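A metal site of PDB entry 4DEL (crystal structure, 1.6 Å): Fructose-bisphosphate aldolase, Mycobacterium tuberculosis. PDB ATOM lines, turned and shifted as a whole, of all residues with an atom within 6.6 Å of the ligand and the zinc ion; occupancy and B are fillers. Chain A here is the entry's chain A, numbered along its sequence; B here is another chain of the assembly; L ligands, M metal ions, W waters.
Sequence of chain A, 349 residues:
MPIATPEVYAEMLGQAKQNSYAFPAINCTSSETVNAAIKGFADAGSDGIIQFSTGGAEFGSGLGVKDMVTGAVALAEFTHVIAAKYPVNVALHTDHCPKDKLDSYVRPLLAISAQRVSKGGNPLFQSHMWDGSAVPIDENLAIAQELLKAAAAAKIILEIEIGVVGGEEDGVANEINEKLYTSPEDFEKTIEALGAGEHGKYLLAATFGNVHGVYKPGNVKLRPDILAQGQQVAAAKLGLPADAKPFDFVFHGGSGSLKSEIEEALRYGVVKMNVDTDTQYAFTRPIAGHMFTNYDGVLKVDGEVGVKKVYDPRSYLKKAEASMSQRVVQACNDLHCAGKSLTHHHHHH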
ATOM      1  N   ALA A  25     -18.883  25.663   9.010  1.00  0.00           N
ATOM      2  CA  ALA A  25     -18.106  25.446  10.225  1.00  0.00           C
ATOM      3  C   ALA A  25     -17.152  24.302   9.887  1.00  0.00           C
ATOM      4  O   ALA A  25     -17.585  23.163   9.731  1.00  0.00           O
ATOM      5  CB  ALA A  25     -19.003  25.092  11.403  1.00  0.00           C
ATOM      6  N   ASN A  27     -14.137  21.752  10.424  1.00  0.00           N
ATOM      7  CA  ASN A  27     -13.321  21.092  11.436  1.00  0.00           C
ATOM      8  C   ASN A  27     -11.848  21.214  11.063  1.00  0.00           C
ATOM      9  O   ASN A  27     -11.483  20.926   9.914  1.00  0.00           O
ATOM     10  CB  ASN A  27     -13.677  19.618  11.600  1.00  0.00           C
ATOM     11  CG  ASN A  27     -14.996  19.426  12.318  1.00  0.00           C
ATOM     12  OD1 ASN A  27     -16.063  19.570  11.713  1.00  0.00           O
ATOM     13  ND2 ASN A  27     -14.918  19.121  13.609  1.00  0.00           N
ATOM     14  N   GLN A  51     -13.846  25.033  13.836  1.00  0.00           N
ATOM     15  CA  GLN A  51     -14.229  24.202  14.975  1.00  0.00           C
ATOM     16  C   GLN A  51     -13.269  23.053  15.241  1.00  0.00           C
ATOM     17  O   GLN A  51     -12.660  22.500  14.305  1.00  0.00           O
ATOM     18  CB  GLN A  51     -15.695  23.734  14.870  1.00  0.00           C
ATOM     19  CG  GLN A  51     -16.036  22.823  13.707  1.00  0.00           C
ATOM     20  CD  GLN A  51     -17.529  22.436  13.674  1.00  0.00           C
ATOM     21  OE1 GLN A  51     -18.403  23.201  14.106  1.00  0.00           O
ATOM     22  NE2 GLN A  51     -17.818  21.264  13.140  1.00  0.00           N
ATOM     23  N   ASP A  95     -16.719  21.300  18.725  1.00  0.00           N
ATOM     24  CA  ASP A  95     -17.708  20.363  18.196  1.00  0.00           C
ATOM     25  C   ASP A  95     -18.097  19.305  19.263  1.00  0.00           C
ATOM     26  O   ASP A  95     -17.622  19.365  20.403  1.00  0.00           O
ATOM     27  CB  ASP A  95     -17.113  19.692  16.948  1.00  0.00           C
ATOM     28  CG  ASP A  95     -18.169  19.208  15.952  1.00  0.00           C
ATOM     29  OD1 ASP A  95     -19.382  19.460  16.106  1.00  0.00           O
ATOM     30  OD2 ASP A  95     -17.780  18.524  14.978  1.00  0.00           O
ATOM     31  N   HIS A  96     -18.977  18.369  18.875  1.00  0.00           N
ATOM     32  CA  HIS A  96     -19.592  17.344  19.753  1.00  0.00           C
ATOM     33  C   HIS A  96     -18.878  17.055  21.075  1.00  0.00           C
ATOM     34  O   HIS A  96     -17.806  16.440  21.101  1.00  0.00           O
ATOM     35  CB  HIS A  96     -19.778  15.997  19.023  1.00  0.00           C
ATOM     36  CG  HIS A  96     -20.559  16.087  17.750  1.00  0.00           C
ATOM     37  ND1 HIS A  96     -21.922  15.909  17.706  1.00  0.00           N
ATOM     38  CD2 HIS A  96     -20.170  16.328  16.482  1.00  0.00           C
ATOM     39  CE1 HIS A  96     -22.337  16.022  16.456  1.00  0.00           C
ATOM     40  NE2 HIS A  96     -21.288  16.284  15.690  1.00  0.00           N
ATOM     41  N   MET A 129     -20.179  23.441  21.662  1.00  0.00           N
ATOM     42  CA  MET A 129     -21.252  22.478  21.492  1.00  0.00           C
ATOM     43  C   MET A 129     -21.406  21.510  22.668  1.00  0.00           C
ATOM     44  O   MET A 129     -20.461  20.805  23.055  1.00  0.00           O
ATOM     45  CB  MET A 129     -21.092  21.652  20.205  1.00  0.00           C
ATOM     46  CG  MET A 129     -22.318  20.802  19.930  1.00  0.00           C
ATOM     47  SD  MET A 129     -22.167  19.621  18.587  1.00  0.00           S
ATOM     48  CE  MET A 129     -23.898  19.131  18.444  1.00  0.00           C
ATOM     49  N   GLU A 159     -24.213  25.702  21.364  1.00  0.00           N
ATOM     50  CA  GLU A 159     -24.900  24.816  20.434  1.00  0.00           C
ATOM     51  C   GLU A 159     -25.307  23.555  21.191  1.00  0.00           C
ATOM     52  O   GLU A 159     -24.522  22.999  21.964  1.00  0.00           O
ATOM     53  CB  GLU A 159     -23.963  24.449  19.264  1.00  0.00           C
ATOM     54  CG  GLU A 159     -24.648  23.581  18.187  1.00  0.00           C
ATOM     55  CD  GLU A 159     -23.701  23.218  17.057  1.00  0.00           C
ATOM     56  OE1 GLU A 159     -22.960  24.113  16.583  1.00  0.00           O
ATOM     57  OE2 GLU A 159     -23.720  22.045  16.613  1.00  0.00           O
ATOM     58  N   GLU A 161     -27.740  19.673  20.754  1.00  0.00           N
ATOM     59  CA  GLU A 161     -28.246  18.741  19.751  1.00  0.00           C
ATOM     60  C   GLU A 161     -29.436  17.963  20.279  1.00  0.00           C
ATOM     61  O   GLU A 161     -29.387  17.430  21.396  1.00  0.00           O
ATOM     62  CB  GLU A 161     -27.155  17.742  19.310  1.00  0.00           C
ATOM     63  CG  GLU A 161     -27.612  16.747  18.248  1.00  0.00           C
ATOM     64  CD  GLU A 161     -26.499  15.855  17.716  1.00  0.00           C
ATOM     65  OE1 GLU A 161     -25.396  16.373  17.498  1.00  0.00           O
ATOM     66  OE2 GLU A 161     -26.748  14.639  17.502  1.00  0.00           O
ATOM     67  N   VAL A 165     -26.953  12.117  15.176  1.00  0.00           N
ATOM     68  CA  VAL A 165     -26.313  12.127  13.857  1.00  0.00           C
ATOM     69  C   VAL A 165     -25.764  10.727  13.615  1.00  0.00           C
ATOM     70  O   VAL A 165     -25.073  10.190  14.472  1.00  0.00           O
ATOM     71  CB  VAL A 165     -25.179  13.181  13.757  1.00  0.00           C
ATOM     72  CG1 VAL A 165     -24.560  13.183  12.359  1.00  0.00           C
ATOM     73  CG2 VAL A 165     -25.704  14.575  14.095  1.00  0.00           C
ATOM     74  N   GLU A 169     -17.887   8.934  14.351  1.00  0.00           N
ATOM     75  CA  GLU A 169     -17.215  10.159  14.750  1.00  0.00           C
ATOM     76  C   GLU A 169     -16.297   9.859  15.866  1.00  0.00           C
ATOM     77  O   GLU A 169     -16.696   9.709  16.997  1.00  0.00           O
ATOM     78  CB  GLU A 169     -18.153  11.280  15.056  1.00  0.00           C
ATOM     79  CG  GLU A 169     -18.286  12.212  13.939  1.00  0.00           C
ATOM     80  CD  GLU A 169     -17.060  12.257  13.057  1.00  0.00           C
ATOM     81  OE1 GLU A 169     -16.081  12.863  13.434  1.00  0.00           O
ATOM     82  OE2 GLU A 169     -17.053  11.649  11.988  1.00  0.00           O
ATOM     83  N   VAL A 211     -25.950  12.307   8.505  1.00  0.00           N
ATOM     84  CA  VAL A 211     -24.945  11.282   8.723  1.00  0.00           C
ATOM     85  C   VAL A 211     -23.547  11.889   8.550  1.00  0.00           C
ATOM     86  O   VAL A 211     -23.287  12.530   7.518  1.00  0.00           O
ATOM     87  CB  VAL A 211     -25.137  10.071   7.754  1.00  0.00           C
ATOM     88  CG1 VAL A 211     -24.039   9.047   7.940  1.00  0.00           C
ATOM     89  CG2 VAL A 211     -26.501   9.408   7.960  1.00  0.00           C
ATOM     90  N   HIS A 212     -22.681  11.694   9.539  1.00  0.00           N
ATOM     91  CA  HIS A 212     -21.284  12.128   9.457  1.00  0.00           C
ATOM     92  C   HIS A 212     -20.585  11.241   8.425  1.00  0.00           C
ATOM     93  O   HIS A 212     -20.753  10.014   8.434  1.00  0.00           O
ATOM     94  CB  HIS A 212     -20.604  11.937  10.805  1.00  0.00           C
ATOM     95  CG  HIS A 212     -20.970  12.973  11.825  1.00  0.00           C
ATOM     96  ND1 HIS A 212     -21.310  12.645  13.130  1.00  0.00           N
ATOM     97  CD2 HIS A 212     -21.037  14.323  11.749  1.00  0.00           C
ATOM     98  CE1 HIS A 212     -21.548  13.750  13.810  1.00  0.00           C
ATOM     99  NE2 HIS A 212     -21.404  14.781  12.998  1.00  0.00           N
ATOM    100  N   GLY A 213     -19.796  11.868   7.558  1.00  0.00           N
ATOM    101  CA  GLY A 213     -19.017  11.126   6.548  1.00  0.00           C
ATOM    102  C   GLY A 213     -19.537  11.345   5.134  1.00  0.00           C
ATOM    103  O   GLY A 213     -20.432  12.182   4.905  1.00  0.00           O
ATOM    104  N   VAL A 214     -18.955  10.603   4.185  1.00  0.00           N
ATOM    105  CA  VAL A 214     -19.287  10.736   2.767  1.00  0.00           C
ATOM    106  C   VAL A 214     -19.536   9.351   2.196  1.00  0.00           C
ATOM    107  O   VAL A 214     -18.631   8.521   2.133  1.00  0.00           O
ATOM    108  CB  VAL A 214     -18.191  11.500   1.970  1.00  0.00           C
ATOM    109  CG1 VAL A 214     -18.414  11.419   0.453  1.00  0.00           C
ATOM    110  CG2 VAL A 214     -18.132  12.967   2.405  1.00  0.00           C
ATOM    111  N   PHE A 251     -26.723  22.354  10.632  1.00  0.00           N
ATOM    112  CA  PHE A 251     -26.744  21.232   9.666  1.00  0.00           C
ATOM    113  C   PHE A 251     -25.436  20.412   9.857  1.00  0.00           C
ATOM    114  O   PHE A 251     -24.364  20.820   9.389  1.00  0.00           O
ATOM    115  CB  PHE A 251     -26.789  21.858   8.255  1.00  0.00           C
ATOM    116  CG  PHE A 251     -27.037  20.890   7.105  1.00  0.00           C
ATOM    117  CD1 PHE A 251     -26.453  19.614   7.069  1.00  0.00           C
ATOM    118  CD2 PHE A 251     -27.765  21.325   5.989  1.00  0.00           C
ATOM    119  CE1 PHE A 251     -26.656  18.767   5.974  1.00  0.00           C
ATOM    120  CE2 PHE A 251     -27.974  20.486   4.885  1.00  0.00           C
ATOM    121  CZ  PHE A 251     -27.401  19.204   4.882  1.00  0.00           C
ATOM    122  N   HIS A 252     -25.547  19.300  10.584  1.00  0.00           N
ATOM    123  CA  HIS A 252     -24.411  18.363  10.758  1.00  0.00           C
ATOM    124  C   HIS A 252     -24.283  17.397   9.581  1.00  0.00           C
ATOM    125  O   HIS A 252     -25.232  17.197   8.809  1.00  0.00           O
ATOM    126  CB  HIS A 252     -24.492  17.574  12.077  1.00  0.00           C
ATOM    127  CG  HIS A 252     -24.094  18.381  13.279  1.00  0.00           C
ATOM    128  ND1 HIS A 252     -22.968  18.125  14.019  1.00  0.00           N
ATOM    129  CD2 HIS A 252     -24.703  19.445  13.870  1.00  0.00           C
ATOM    130  CE1 HIS A 252     -22.877  19.006  15.009  1.00  0.00           C
ATOM    131  NE2 HIS A 252     -23.927  19.812  14.936  1.00  0.00           N
ATOM    132  N   GLY A 253     -23.109  16.799   9.444  1.00  0.00           N
ATOM    133  CA  GLY A 253     -22.877  15.857   8.355  1.00  0.00           C
ATOM    134  C   GLY A 253     -22.963  16.495   6.984  1.00  0.00           C
ATOM    135  O   GLY A 253     -23.393  15.850   6.027  1.00  0.00           O
ATOM    136  N   GLY A 254     -22.540  17.764   6.878  1.00  0.00           N
ATOM    137  CA  GLY A 254     -22.631  18.521   5.629  1.00  0.00           C
ATOM    138  C   GLY A 254     -21.947  17.915   4.398  1.00  0.00           C
ATOM    139  O   GLY A 254     -22.476  17.969   3.293  1.00  0.00           O
ATOM    140  N   SER A 255     -20.794  17.289   4.616  1.00  0.00           N
ATOM    141  CA  SER A 255     -20.047  16.720   3.483  1.00  0.00           C
ATOM    142  C   SER A 255     -20.882  15.695   2.734  1.00  0.00           C
ATOM    143  O   SER A 255     -21.574  14.903   3.351  1.00  0.00           O
ATOM    144  CB  SER A 255     -18.791  16.014   3.995  1.00  0.00           C
ATOM    145  OG  SER A 255     -17.914  16.922   4.640  1.00  0.00           O
ATOM    146  N   GLY A 256     -20.777  15.695   1.404  1.00  0.00           N
ATOM    147  CA  GLY A 256     -21.441  14.688   0.585  1.00  0.00           C
ATOM    148  C   GLY A 256     -22.918  14.941   0.334  1.00  0.00           C
ATOM    149  O   GLY A 256     -23.576  14.167  -0.377  1.00  0.00           O
ATOM    150  N   ASN A 274     -21.874  22.206   9.218  1.00  0.00           N
ATOM    151  CA  ASN A 274     -20.592  21.621   9.596  1.00  0.00           C
ATOM    152  C   ASN A 274     -20.039  20.825   8.427  1.00  0.00           C
ATOM    153  O   ASN A 274     -20.770  20.030   7.814  1.00  0.00           O
ATOM    154  CB  ASN A 274     -20.770  20.677  10.802  1.00  0.00           C
ATOM    155  CG  ASN A 274     -21.081  21.410  12.121  1.00  0.00           C
ATOM    156  OD1 ASN A 274     -21.002  20.803  13.203  1.00  0.00           O
ATOM    157  ND2 ASN A 274     -21.434  22.676  12.039  1.00  0.00           N
ATOM    158  N   VAL A 275     -18.755  21.031   8.132  1.00  0.00           N
ATOM    159  CA  VAL A 275     -18.044  20.301   7.073  1.00  0.00           C
ATOM    160  C   VAL A 275     -16.723  19.791   7.651  1.00  0.00           C
ATOM    161  O   VAL A 275     -15.961  20.559   8.252  1.00  0.00           O
ATOM    162  CB  VAL A 275     -17.793  21.220   5.858  1.00  0.00           C
ATOM    163  CG1 VAL A 275     -16.881  20.544   4.825  1.00  0.00           C
ATOM    164  CG2 VAL A 275     -19.151  21.631   5.204  1.00  0.00           C
ATOM    165  N   ASP A 276     -16.481  18.491   7.512  1.00  0.00           N
ATOM    166  CA  ASP A 276     -15.216  17.899   7.981  1.00  0.00           C
ATOM    167  C   ASP A 276     -14.706  16.920   6.934  1.00  0.00           C
ATOM    168  O   ASP A 276     -13.643  17.132   6.349  1.00  0.00           O
ATOM    169  CB  ASP A 276     -15.397  17.230   9.350  1.00  0.00           C
ATOM    170  CG  ASP A 276     -14.080  16.875  10.029  1.00  0.00           C
ATOM    171  OD1 ASP A 276     -12.988  17.097   9.422  1.00  0.00           O
ATOM    172  OD2 ASP A 276     -14.120  16.405  11.200  1.00  0.00           O
ATOM    173  N   THR A 277     -15.493  15.874   6.669  1.00  0.00           N
ATOM    174  CA  THR A 277     -15.034  14.791   5.779  1.00  0.00           C
ATOM    175  C   THR A 277     -14.572  15.275   4.389  1.00  0.00           C
ATOM    176  O   THR A 277     -13.520  14.849   3.891  1.00  0.00           O
ATOM    177  CB  THR A 277     -16.093  13.682   5.659  1.00  0.00           C
ATOM    178  OG1 THR A 277     -16.445  13.213   6.963  1.00  0.00           O
ATOM    179  CG2 THR A 277     -15.533  12.495   4.872  1.00  0.00           C
ATOM    180  N   ASP A 278     -15.333  16.188   3.770  1.00  0.00           N
ATOM    181  CA  ASP A 278     -14.989  16.695   2.442  1.00  0.00           C
ATOM    182  C   ASP A 278     -13.728  17.540   2.439  1.00  0.00           C
ATOM    183  O   ASP A 278     -12.947  17.462   1.500  1.00  0.00           O
ATOM    184  CB  ASP A 278     -16.147  17.482   1.816  1.00  0.00           C
ATOM    185  CG  ASP A 278     -17.107  16.584   1.023  1.00  0.00           C
ATOM    186  OD1 ASP A 278     -16.785  15.412   0.749  1.00  0.00           O
ATOM    187  OD2 ASP A 278     -18.196  17.089   0.663  1.00  0.00           O
ATOM    188  N   GLN A 280     -11.331  17.100   4.636  1.00  0.00           N
ATOM    189  CA  GLN A 280     -10.271  16.102   4.862  1.00  0.00           C
ATOM    190  C   GLN A 280      -9.830  15.499   3.526  1.00  0.00           C
ATOM    191  O   GLN A 280      -8.625  15.410   3.236  1.00  0.00           O
ATOM    192  CB  GLN A 280     -10.732  14.995   5.785  1.00  0.00           C
ATOM    193  CG  GLN A 280     -10.981  15.443   7.244  1.00  0.00           C
ATOM    194  CD  GLN A 280     -11.329  14.283   8.148  1.00  0.00           C
ATOM    195  OE1 GLN A 280     -11.119  14.346   9.367  1.00  0.00           O
ATOM    196  NE2 GLN A 280     -11.879  13.238   7.568  1.00  0.00           N
ATOM    197  N   LYS B 308     -12.666   7.243   4.630  1.00  0.00           N
ATOM    198  CA  LYS B 308     -12.362   8.360   5.521  1.00  0.00           C
ATOM    199  C   LYS B 308     -11.312   8.035   6.565  1.00  0.00           C
ATOM    200  O   LYS B 308     -10.483   8.909   6.881  1.00  0.00           O
ATOM    201  CB  LYS B 308     -13.638   8.857   6.219  1.00  0.00           C
ATOM    202  CG  LYS B 308     -13.416   9.923   7.294  1.00  0.00           C
ATOM    203  CD  LYS B 308     -14.722  10.238   8.031  1.00  0.00           C
ATOM    204  CE  LYS B 308     -14.499  11.136   9.233  1.00  0.00           C
ATOM    205  NZ  LYS B 308     -14.406  12.571   8.863  1.00  0.00           N
HETATM  206  C1  LIG L   1     -19.846  17.434  11.200  1.00  0.00           C
HETATM  207  C2  LIG L   1     -19.275  17.300   9.820  1.00  0.00           C
HETATM  208  N1  LIG L   1     -19.048  17.606  12.224  1.00  0.00           N
HETATM  209  O1  LIG L   1     -19.600  17.749  13.469  1.00  0.00           O
HETATM  210  O2  LIG L   1     -21.213  17.366  11.344  1.00  0.00           O
HETATM  211  O3  LIG L   1     -19.883  16.202   9.158  1.00  0.00           O
HETATM  212  O4  LIG L   1     -20.124  14.721   7.099  1.00  0.00           O
HETATM  213  O5  LIG L   1     -19.008  16.924   6.933  1.00  0.00           O
HETATM  214  O6  LIG L   1     -17.868  15.050   8.157  1.00  0.00           O
HETATM  215  P1  LIG L   1     -19.196  15.691   7.787  1.00  0.00           P
HETATM  216 ZN    ZN M   1     -21.427  16.771  13.608  1.00  0.00          ZN
HETATM  217  O   HOH W   1     -17.185  13.788  10.405  1.00  0.00           O
HETATM  218  O   HOH W   2     -16.605  16.094  12.326  1.00  0.00           O
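Three residues have an atom within 4 Å of the zinc ion: His 96, His 212 and His 252.
The nearest printed residue that does not touch the zinc ion is Asn 274 (4.1 Å).
N1 of the ligand lies within hydrogen-bond range of OD2 of Asp 95 (3.2 Å).
N of Ser 255 sits at hydrogen-bond distance from O5 of the ligand, at 2.9 Å.
An oxygen (O5) of the ligand is in hydrogen-bond range of the side-chain hydroxyl (OG) of Ser 255 (2.5 Å).
N of Thr 277 sits at hydrogen-bond distance from O6 of the ligand.
O6 of the ligand lies within hydrogen-bond range of OG1 of Thr 277 (2.6 Å).
O3 of the ligand lies close to N of Gly 253 (3.3 Å).
N of Gly 213 lies within hydrogen-bond range of O4 of the ligand, at 2.9 Å.
An oxygen (O5) of the ligand is in hydrogen-bond range of the backbone NH (N) of Asp 276 (3.0 Å).
The side-chain amide oxygen of Asn 274 sits close to an oxygen (O1) of the ligand (3.4 Å).
The zinc ion is bound by an oxygen (O1) of the ligand (2.1 Å), a ring nitrogen (NE2) of His 212 (2.1 Å), a ring nitrogen (ND1) of His 252 (2.1 Å), a ring nitrogen (NE2) of His 96 (2.1 Å) and an oxygen (O2) of the ligand (2.4 Å).
The zinc ion has five donor atoms within binding distance.
Water W1 lies within hydrogen-bond range of OE2 of Glu 169 (2.7 Å), O6 of the ligand (2.7 Å) and NZ of Lys 308 of chain B (3.4 Å).
Water W2 lies within hydrogen-bond range of OD2 of Asp 276, N1 of the ligand and OE1 of Glu 169.
Residues that only touch the ligand: Asn 27 (3.6 Å), Gln 51 (3.95 Å), Val 211 (3.9 Å), Gly 254 (3.6 Å) and Val 275 (3.5 Å).
Hydrophobic or aromatic side chains within 4 Å of the ligand: His 96, His 212 and His 252.
Of the 27 residues printed, 15 come within 4 Å of the ligand.
A ring nitrogen (ND1) of His 252 sits close to the side-chain amide oxygen of Asn 274.
A ring nitrogen (NE2) of His 252 sits at hydrogen-bond distance from the side-chain carboxylate of Glu 159 (2.8 Å).
The backbone NH of His 96 is in hydrogen-bond range of the side-chain sulfur of Met 129.
The side-chain amide nitrogen (ND2) of Asn 27 sits at hydrogen-bond distance from the side-chain carboxylate (OD2) of Asp 95 (3.2 Å).
OG of Ser 255 sits at hydrogen-bond distance from N of Thr 277, at 3.3 Å.
N of Asp 278 lies within hydrogen-bond range of OG of Ser 255, 2.8 Å away.
OD1 of Asn 274 sits at hydrogen-bond distance from NE2 of Gln 51, 3.2 Å away.
NE2 of Gln 51 lies within hydrogen-bond range of OD1 of Asn 27, at 2.8 Å.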
